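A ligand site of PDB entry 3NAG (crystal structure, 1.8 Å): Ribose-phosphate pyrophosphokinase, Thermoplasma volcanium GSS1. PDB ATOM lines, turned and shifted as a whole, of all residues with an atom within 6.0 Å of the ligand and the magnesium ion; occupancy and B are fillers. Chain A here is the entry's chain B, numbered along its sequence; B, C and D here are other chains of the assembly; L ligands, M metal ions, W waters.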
ATOM      1  N   TYR A  89      20.925  -6.232  12.306  1.00  0.00           N
ATOM      2  CA  TYR A  89      20.321  -4.939  11.948  1.00  0.00           C
ATOM      3  C   TYR A  89      21.279  -3.931  11.339  1.00  0.00           C
ATOM      4  O   TYR A  89      20.940  -2.761  11.161  1.00  0.00           O
ATOM      5  CB  TYR A  89      19.550  -4.329  13.128  1.00  0.00           C
ATOM      6  CG  TYR A  89      18.332  -5.155  13.442  1.00  0.00           C
ATOM      7  CD1 TYR A  89      17.144  -4.929  12.768  1.00  0.00           C
ATOM      8  CD2 TYR A  89      18.384  -6.184  14.383  1.00  0.00           C
ATOM      9  CE1 TYR A  89      16.014  -5.674  13.038  1.00  0.00           C
ATOM     10  CE2 TYR A  89      17.264  -6.963  14.641  1.00  0.00           C
ATOM     11  CZ  TYR A  89      16.076  -6.695  13.960  1.00  0.00           C
ATOM     12  OH  TYR A  89      14.949  -7.453  14.209  1.00  0.00           O
ATOM     13  N   ARG A  91      22.090  -3.818   8.446  1.00  0.00           N
ATOM     14  CA  ARG A  91      21.574  -3.466   7.131  1.00  0.00           C
ATOM     15  C   ARG A  91      20.621  -2.289   7.215  1.00  0.00           C
ATOM     16  O   ARG A  91      20.404  -1.585   6.220  1.00  0.00           O
ATOM     17  CB  ARG A  91      20.843  -4.644   6.495  1.00  0.00           C
ATOM     18  CG  ARG A  91      21.725  -5.781   6.044  1.00  0.00           C
ATOM     19  CD  ARG A  91      21.246  -6.246   4.687  1.00  0.00           C
ATOM     20  NE  ARG A  91      21.245  -7.696   4.557  1.00  0.00           N
ATOM     21  CZ  ARG A  91      20.842  -8.337   3.466  1.00  0.00           C
ATOM     22  NH1 ARG A  91      20.434  -7.659   2.397  1.00  0.00           N
ATOM     23  NH2 ARG A  91      20.865  -9.663   3.440  1.00  0.00           N
ATOM     24  N   GLN A  92      20.045  -2.070   8.389  1.00  0.00           N
ATOM     25  CA  GLN A  92      19.151  -0.933   8.613  1.00  0.00           C
ATOM     26  C   GLN A  92      19.893   0.134   9.416  1.00  0.00           C
ATOM     27  O   GLN A  92      19.605   0.351  10.609  1.00  0.00           O
ATOM     28  CB  GLN A  92      17.866  -1.380   9.340  1.00  0.00           C
ATOM     29  CG  GLN A  92      16.823  -0.288   9.513  1.00  0.00           C
ATOM     30  CD  GLN A  92      16.190   0.137   8.199  1.00  0.00           C
ATOM     31  OE1 GLN A  92      16.338  -0.549   7.180  1.00  0.00           O
ATOM     32  NE2 GLN A  92      15.486   1.263   8.223  1.00  0.00           N
ATOM     33  N   HIS A  93      20.860   0.782   8.776  1.00  0.00           N
ATOM     34  CA  HIS A  93      21.742   1.719   9.457  1.00  0.00           C
ATOM     35  C   HIS A  93      21.411   3.172   9.128  1.00  0.00           C
ATOM     36  O   HIS A  93      22.181   4.071   9.451  1.00  0.00           O
ATOM     37  CB  HIS A  93      23.205   1.422   9.091  1.00  0.00           C
ATOM     38  CG  HIS A  93      23.445   1.305   7.618  1.00  0.00           C
ATOM     39  ND1 HIS A  93      23.642   2.413   6.808  1.00  0.00           N
ATOM     40  CD2 HIS A  93      23.490   0.230   6.800  1.00  0.00           C
ATOM     41  CE1 HIS A  93      23.815   2.016   5.559  1.00  0.00           C
ATOM     42  NE2 HIS A  93      23.734   0.699   5.528  1.00  0.00           N
ATOM     43  N   GLN A  94      20.274   3.376   8.475  1.00  0.00           N
ATOM     44  CA  GLN A  94      19.740   4.706   8.212  1.00  0.00           C
ATOM     45  C   GLN A  94      18.277   4.544   7.826  1.00  0.00           C
ATOM     46  O   GLN A  94      17.815   3.421   7.616  1.00  0.00           O
ATOM     47  CB  GLN A  94      20.495   5.368   7.059  1.00  0.00           C
ATOM     48  CG  GLN A  94      20.453   4.554   5.792  1.00  0.00           C
ATOM     49  CD  GLN A  94      20.862   5.343   4.582  1.00  0.00           C
ATOM     50  OE1 GLN A  94      22.054   5.499   4.288  1.00  0.00           O
ATOM     51  NE2 GLN A  94      19.873   5.860   3.857  1.00  0.00           N
ATOM     52  N   TYR A  96      15.491   4.804   5.025  1.00  0.00           N
ATOM     53  CA  TYR A  96      15.384   4.827   3.574  1.00  0.00           C
ATOM     54  C   TYR A  96      14.016   5.333   3.144  1.00  0.00           C
ATOM     55  O   TYR A  96      13.799   5.673   1.973  1.00  0.00           O
ATOM     56  CB  TYR A  96      15.668   3.435   2.978  1.00  0.00           C
ATOM     57  CG  TYR A  96      17.026   2.878   3.375  1.00  0.00           C
ATOM     58  CD1 TYR A  96      18.116   2.978   2.532  1.00  0.00           C
ATOM     59  CD2 TYR A  96      17.209   2.262   4.606  1.00  0.00           C
ATOM     60  CE1 TYR A  96      19.366   2.475   2.894  1.00  0.00           C
ATOM     61  CE2 TYR A  96      18.453   1.765   4.984  1.00  0.00           C
ATOM     62  CZ  TYR A  96      19.517   1.864   4.117  1.00  0.00           C
ATOM     63  OH  TYR A  96      20.752   1.375   4.488  1.00  0.00           O
ATOM     64  N   GLU A 100      10.758   5.048   9.138  1.00  0.00           N
ATOM     65  CA  GLU A 100      11.465   3.780   9.392  1.00  0.00           C
ATOM     66  C   GLU A 100      12.338   3.922  10.630  1.00  0.00           C
ATOM     67  O   GLU A 100      12.764   5.022  10.957  1.00  0.00           O
ATOM     68  CB  GLU A 100      12.342   3.403   8.195  1.00  0.00           C
ATOM     69  CG  GLU A 100      11.595   2.881   6.959  1.00  0.00           C
ATOM     70  CD  GLU A 100      12.561   2.406   5.876  1.00  0.00           C
ATOM     71  OE1 GLU A 100      13.781   2.554   6.065  1.00  0.00           O
ATOM     72  OE2 GLU A 100      12.088   1.892   4.845  1.00  0.00           O
ATOM     73  N   HIS A 124      28.225  -4.997   8.489  1.00  0.00           N
ATOM     74  CA  HIS A 124      27.799  -4.764   7.108  1.00  0.00           C
ATOM     75  C   HIS A 124      28.041  -3.337   6.613  1.00  0.00           C
ATOM     76  O   HIS A 124      28.289  -3.139   5.427  1.00  0.00           O
ATOM     77  CB  HIS A 124      26.341  -5.139   6.894  1.00  0.00           C
ATOM     78  CG  HIS A 124      25.869  -4.882   5.505  1.00  0.00           C
ATOM     79  ND1 HIS A 124      26.335  -5.592   4.419  1.00  0.00           N
ATOM     80  CD2 HIS A 124      25.009  -3.950   5.011  1.00  0.00           C
ATOM     81  CE1 HIS A 124      25.764  -5.129   3.319  1.00  0.00           C
ATOM     82  NE2 HIS A 124      24.957  -4.135   3.652  1.00  0.00           N
ATOM     83  N   ASP A 125      27.949  -2.361   7.497  1.00  0.00           N
ATOM     84  CA  ASP A 125      28.313  -0.978   7.150  1.00  0.00           C
ATOM     85  C   ASP A 125      28.820  -0.263   8.395  1.00  0.00           C
ATOM     86  O   ASP A 125      28.150  -0.242   9.430  1.00  0.00           O
ATOM     87  CB  ASP A 125      27.099  -0.243   6.581  1.00  0.00           C
ATOM     88  CG  ASP A 125      27.457   1.124   6.009  1.00  0.00           C
ATOM     89  OD1 ASP A 125      27.047   1.402   4.860  1.00  0.00           O
ATOM     90  OD2 ASP A 125      28.130   1.912   6.703  1.00  0.00           O
ATOM     91  N   SER A 214      22.738 -14.186   2.605  1.00  0.00           N
ATOM     92  CA  SER A 214      21.400 -14.423   3.134  1.00  0.00           C
ATOM     93  C   SER A 214      20.551 -15.190   2.110  1.00  0.00           C
ATOM     94  O   SER A 214      20.506 -16.420   2.135  1.00  0.00           O
ATOM     95  CB  SER A 214      20.740 -13.115   3.609  1.00  0.00           C
ATOM     96  OG  SER A 214      20.592 -12.196   2.550  1.00  0.00           O
ATOM     97  N   ARG B  30       6.754  -6.107   8.552  1.00  0.00           N
ATOM     98  CA  ARG B  30       7.014  -7.407   7.967  1.00  0.00           C
ATOM     99  C   ARG B  30       8.370  -7.882   8.454  1.00  0.00           C
ATOM    100  O   ARG B  30       9.115  -7.129   9.077  1.00  0.00           O
ATOM    101  CB  ARG B  30       6.997  -7.344   6.435  1.00  0.00           C
ATOM    102  CG  ARG B  30       8.227  -6.721   5.823  1.00  0.00           C
ATOM    103  CD  ARG B  30       8.113  -6.639   4.304  1.00  0.00           C
ATOM    104  NE  ARG B  30       9.327  -6.057   3.726  1.00  0.00           N
ATOM    105  CZ  ARG B  30       9.509  -4.750   3.534  1.00  0.00           C
ATOM    106  NH1 ARG B  30       8.559  -3.898   3.884  1.00  0.00           N
ATOM    107  NH2 ARG B  30      10.641  -4.307   3.009  1.00  0.00           N
ATOM    108  N   PHE B  32      12.085  -9.301   7.274  1.00  0.00           N
ATOM    109  CA  PHE B  32      13.023  -9.495   6.183  1.00  0.00           C
ATOM    110  C   PHE B  32      13.284 -10.984   5.988  1.00  0.00           C
ATOM    111  O   PHE B  32      12.972 -11.796   6.860  1.00  0.00           O
ATOM    112  CB  PHE B  32      14.334  -8.771   6.494  1.00  0.00           C
ATOM    113  CG  PHE B  32      14.248  -7.264   6.376  1.00  0.00           C
ATOM    114  CD1 PHE B  32      14.088  -6.672   5.129  1.00  0.00           C
ATOM    115  CD2 PHE B  32      14.355  -6.451   7.486  1.00  0.00           C
ATOM    116  CE1 PHE B  32      14.021  -5.283   5.005  1.00  0.00           C
ATOM    117  CE2 PHE B  32      14.298  -5.065   7.361  1.00  0.00           C
ATOM    118  CZ  PHE B  32      14.125  -4.490   6.127  1.00  0.00           C
ATOM    119  N   PRO B  33      13.838 -11.373   4.835  1.00  0.00           N
ATOM    120  CA  PRO B  33      14.068 -12.792   4.591  1.00  0.00           C
ATOM    121  C   PRO B  33      14.900 -13.450   5.692  1.00  0.00           C
ATOM    122  O   PRO B  33      14.669 -14.614   6.024  1.00  0.00           O
ATOM    123  CB  PRO B  33      14.806 -12.807   3.249  1.00  0.00           C
ATOM    124  CG  PRO B  33      14.315 -11.566   2.570  1.00  0.00           C
ATOM    125  CD  PRO B  33      14.182 -10.544   3.664  1.00  0.00           C
ATOM    126  N   ASP B  34      15.835 -12.701   6.262  1.00  0.00           N
ATOM    127  CA  ASP B  34      16.699 -13.225   7.330  1.00  0.00           C
ATOM    128  C   ASP B  34      16.049 -13.227   8.719  1.00  0.00           C
ATOM    129  O   ASP B  34      16.684 -13.574   9.715  1.00  0.00           O
ATOM    130  CB  ASP B  34      18.038 -12.477   7.371  1.00  0.00           C
ATOM    131  CG  ASP B  34      17.880 -11.011   7.751  1.00  0.00           C
ATOM    132  OD1 ASP B  34      16.752 -10.596   8.094  1.00  0.00           O
ATOM    133  OD2 ASP B  34      18.886 -10.269   7.720  1.00  0.00           O
ATOM    134  N   GLU B  36      14.843 -10.586  10.377  1.00  0.00           N
ATOM    135  CA  GLU B  36      14.853  -9.300  11.068  1.00  0.00           C
ATOM    136  C   GLU B  36      13.529  -8.537  10.875  1.00  0.00           C
ATOM    137  O   GLU B  36      12.874  -8.650   9.844  1.00  0.00           O
ATOM    138  CB  GLU B  36      16.073  -8.455  10.683  1.00  0.00           C
ATOM    139  CG  GLU B  36      17.363  -9.099  11.180  1.00  0.00           C
ATOM    140  CD  GLU B  36      18.582  -8.227  10.968  1.00  0.00           C
ATOM    141  OE1 GLU B  36      18.464  -7.158  10.340  1.00  0.00           O
ATOM    142  OE2 GLU B  36      19.656  -8.634  11.430  1.00  0.00           O
ATOM    143  N   TYR B  38      11.002  -5.427  10.278  1.00  0.00           N
ATOM    144  CA  TYR B  38      10.884  -4.144   9.610  1.00  0.00           C
ATOM    145  C   TYR B  38       9.574  -3.447  10.018  1.00  0.00           C
ATOM    146  O   TYR B  38       8.508  -4.063  10.048  1.00  0.00           O
ATOM    147  CB  TYR B  38      10.915  -4.329   8.082  1.00  0.00           C
ATOM    148  CG  TYR B  38      10.615  -3.058   7.313  1.00  0.00           C
ATOM    149  CD1 TYR B  38      11.640  -2.181   6.964  1.00  0.00           C
ATOM    150  CD2 TYR B  38       9.318  -2.724   6.950  1.00  0.00           C
ATOM    151  CE1 TYR B  38      11.385  -1.018   6.255  1.00  0.00           C
ATOM    152  CE2 TYR B  38       9.044  -1.555   6.245  1.00  0.00           C
ATOM    153  CZ  TYR B  38      10.085  -0.702   5.903  1.00  0.00           C
ATOM    154  OH  TYR B  38       9.830   0.455   5.203  1.00  0.00           O
ATOM    155  N   ARG C  40      18.271   5.013 -10.037  1.00  0.00           N
ATOM    156  CA  ARG C  40      18.971   5.073  -8.756  1.00  0.00           C
ATOM    157  C   ARG C  40      20.451   4.749  -8.936  1.00  0.00           C
ATOM    158  O   ARG C  40      20.799   3.776  -9.595  1.00  0.00           O
ATOM    159  CB  ARG C  40      18.341   4.150  -7.726  1.00  0.00           C
ATOM    160  CG  ARG C  40      19.104   4.118  -6.420  1.00  0.00           C
ATOM    161  CD  ARG C  40      18.402   3.294  -5.361  1.00  0.00           C
ATOM    162  NE  ARG C  40      19.089   3.379  -4.074  1.00  0.00           N
ATOM    163  CZ  ARG C  40      19.740   2.367  -3.499  1.00  0.00           C
ATOM    164  NH1 ARG C  40      19.798   1.184  -4.100  1.00  0.00           N
ATOM    165  NH2 ARG C  40      20.334   2.542  -2.331  1.00  0.00           N
ATOM    166  N   ASP C  42      23.470   3.982  -6.489  1.00  0.00           N
ATOM    167  CA  ASP C  42      23.804   3.784  -5.084  1.00  0.00           C
ATOM    168  C   ASP C  42      25.292   3.957  -4.751  1.00  0.00           C
ATOM    169  O   ASP C  42      25.655   4.098  -3.579  1.00  0.00           O
ATOM    170  CB  ASP C  42      23.232   2.476  -4.507  1.00  0.00           C
ATOM    171  CG  ASP C  42      23.561   1.256  -5.339  1.00  0.00           C
ATOM    172  OD1 ASP C  42      24.683   1.194  -5.893  1.00  0.00           O
ATOM    173  OD2 ASP C  42      22.708   0.346  -5.418  1.00  0.00           O
ATOM    174  N   LYS D  97      15.451   5.861  -1.919  1.00  0.00           N
ATOM    175  CA  LYS D  97      16.547   6.124  -1.010  1.00  0.00           C
ATOM    176  C   LYS D  97      17.540   7.124  -1.590  1.00  0.00           C
ATOM    177  O   LYS D  97      17.138   8.118  -2.215  1.00  0.00           O
ATOM    178  CB  LYS D  97      17.251   4.800  -0.746  1.00  0.00           C
ATOM    179  CG  LYS D  97      16.317   3.622  -0.962  1.00  0.00           C
ATOM    180  CD  LYS D  97      17.055   2.345  -1.299  1.00  0.00           C
ATOM    181  CE  LYS D  97      16.081   1.227  -1.643  1.00  0.00           C
ATOM    182  NZ  LYS D  97      15.154   1.624  -2.746  1.00  0.00           N
HETATM  183  P1  LIG L   1      22.986   0.913   1.646  1.00  0.00           P
HETATM  184  O1  LIG L   1      23.244  -0.339   2.452  1.00  0.00           O
HETATM  185  O2  LIG L   1      22.621   2.131   2.465  1.00  0.00           O
HETATM  186  O3  LIG L   1      24.042   1.186   0.595  1.00  0.00           O
HETATM  187  P2  LIG L   1      21.221  -0.892   0.294  1.00  0.00           P
HETATM  188  O4  LIG L   1      22.469  -1.713   0.020  1.00  0.00           O
HETATM  189  O5  LIG L   1      20.170  -0.728  -0.780  1.00  0.00           O
HETATM  190  O6  LIG L   1      21.674   0.602   0.733  1.00  0.00           O
HETATM  191  O7  LIG L   1      20.419  -1.476   1.474  1.00  0.00           O
HETATM  192  C1  LIG L   1      19.430  -0.767   2.208  1.00  0.00           C
HETATM  193  C2  LIG L   1      18.110  -1.522   2.164  1.00  0.00           C
HETATM  194  O8  LIG L   1      18.190  -2.783   2.822  1.00  0.00           O
HETATM  195  C3  LIG L   1      17.029  -0.708   2.872  1.00  0.00           C
HETATM  196  O9  LIG L   1      15.867  -0.697   2.046  1.00  0.00           O
HETATM  197  C4  LIG L   1      16.721  -1.503   4.124  1.00  0.00           C
HETATM  198  O10 LIG L   1      15.357  -1.321   4.509  1.00  0.00           O
HETATM  199  C5  LIG L   1      17.049  -2.920   3.677  1.00  0.00           C
HETATM  200  N1  LIG L   1      17.300  -3.834   4.821  1.00  0.00           N
HETATM  201  C6  LIG L   1      17.469  -3.491   6.115  1.00  0.00           C
HETATM  202  N2  LIG L   1      17.639  -4.588   6.891  1.00  0.00           N
HETATM  203  C7  LIG L   1      17.561  -5.661   6.088  1.00  0.00           C
HETATM  204  C8  LIG L   1      17.656  -7.128   6.256  1.00  0.00           C
HETATM  205  N3  LIG L   1      17.867  -7.672   7.474  1.00  0.00           N
HETATM  206  N4  LIG L   1      17.508  -7.901   5.148  1.00  0.00           N
HETATM  207  C9  LIG L   1      17.294  -7.365   3.925  1.00  0.00           C
HETATM  208  N5  LIG L   1      17.198  -6.047   3.696  1.00  0.00           N
HETATM  209  C10 LIG L   1      17.319  -5.161   4.723  1.00  0.00           C
HETATM  210 MG    MG M   1      22.213  -2.264   2.109  1.00  0.00          MG
HETATM  211  O   HOH W   1      13.429   0.592   2.972  1.00  0.00           O
HETATM  212  O   HOH W   2      16.207  -5.784   1.161  1.00  0.00           O
HETATM  213  O   HOH W   3      21.472  -4.044   2.883  1.00  0.00           O
HETATM  214  O   HOH W   4      16.991  -4.792   9.724  1.00  0.00           O
HETATM  215  O   HOH W   5      22.189  -2.176   4.194  1.00  0.00           O
HETATM  216  O   HOH W   6      25.829  -0.550   3.000  1.00  0.00           O
HETATM  217  O   HOH W   7      17.182 -10.497   4.838  1.00  0.00           O
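Water W5 bridges the backbone carbonyl oxygen (O) of Arg 91 and a ring nitrogen (NE2) of His 124.
Water W7 bridges N4 of the ligand (2.6 Å) and N of Asp 34 of chain B (2.9 Å).
Water W6 lies within hydrogen-bond range of the side-chain carboxylate (OD1) of Asp 125 (3.0 Å) and an oxygen (O3) of the ligand (3.5 Å).
Water W1 lies within hydrogen-bond range of OE2 of Glu 100 (2.6 Å) and O9 of the ligand (2.9 Å).
Water W4 bridges the side-chain carboxylate of Glu 36 of chain B (2.9 Å) and a nitrogen (N2) of the ligand (2.9 Å).
NE2 of His 124 touches the magnesium ion, 3.7 Å away.
The nearest printed residue that does not touch the magnesium ion is Arg 91 (4.5 Å).
The side-chain carboxylate (OD2) of Asp 34 of chain B sits at hydrogen-bond distance from a nitrogen (N3) of the ligand, 2.8 Å away.
An oxygen (O2) of the ligand lies within hydrogen-bond range of the side-chain hydroxyl (OH) of Tyr 96.
O10 of the ligand lies within hydrogen-bond range of OE1 of Gln 92.
OE1 of Glu 36 of chain B is in hydrogen-bond range of N3 of the ligand, 3.0 Å away.
NE2 of His 93 lies close to O1 of the ligand (3.3 Å).
An oxygen (O5) of the ligand is in salt-bridge range of the guanidinium group of Arg 40 of chain C.
Merely in contact with the ligand: Arg 91, Gln 94 and Phe 32 of chain B.
Hydrophobic or aromatic side chains that line the ligand: His 93, Tyr 96 and Phe 32 of chain B.
Nine residues have an atom within 4 Å of the ligand: Arg 91, Gln 92, His 93, Gln 94, Tyr 96, Phe 32 of chain B, Asp 34 of chain B, Glu 36 of chain B and Arg 40 of chain C.
The nearest printed residue that does not touch the ligand is Lys 97 of chain D (4.2 Å).
OD1 of Asp 34 of chain B lies within hydrogen-bond range of N of Glu 36 of chain B, at 3.0 Å.
OH of Tyr 96 sits at hydrogen-bond distance from O of Arg 91 (3.4 Å).
NE2 of His 93 lies within hydrogen-bond range of OH of Tyr 96, 3.2 Å away.
The backbone carbonyl oxygen (O) of Gln 94 sits at hydrogen-bond distance from the side-chain amide nitrogen (NE2) of Gln 92 (3.2 Å).
NE2 of Gln 92 is in hydrogen-bond range of OE1 of Glu 100, at 3.0 Å.
NH2 of Arg 91 lies within hydrogen-bond range of OG of Ser 214, 2.7 Å away.
A ring nitrogen (NE2) of His 93 sits close to the side-chain carboxylate of Asp 125 (3.5 Å).
The guanidinium group of Arg 40 of chain C lies within salt-bridge range of the side-chain carboxylate of Asp 42 of chain C (3.3 Å).
The magnesium ion is bound by an oxygen (O7) of the ligand (2.1 Å).
The magnesium ion is bound by water W3, at 2.1 Å.
The magnesium ion is bound by water W5, 2.1 Å away.
An oxygen (O4) of the ligand is bound to the magnesium ion, at 2.2 Å.
O1 of the ligand is bound to the magnesium ion (2.2 Å).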
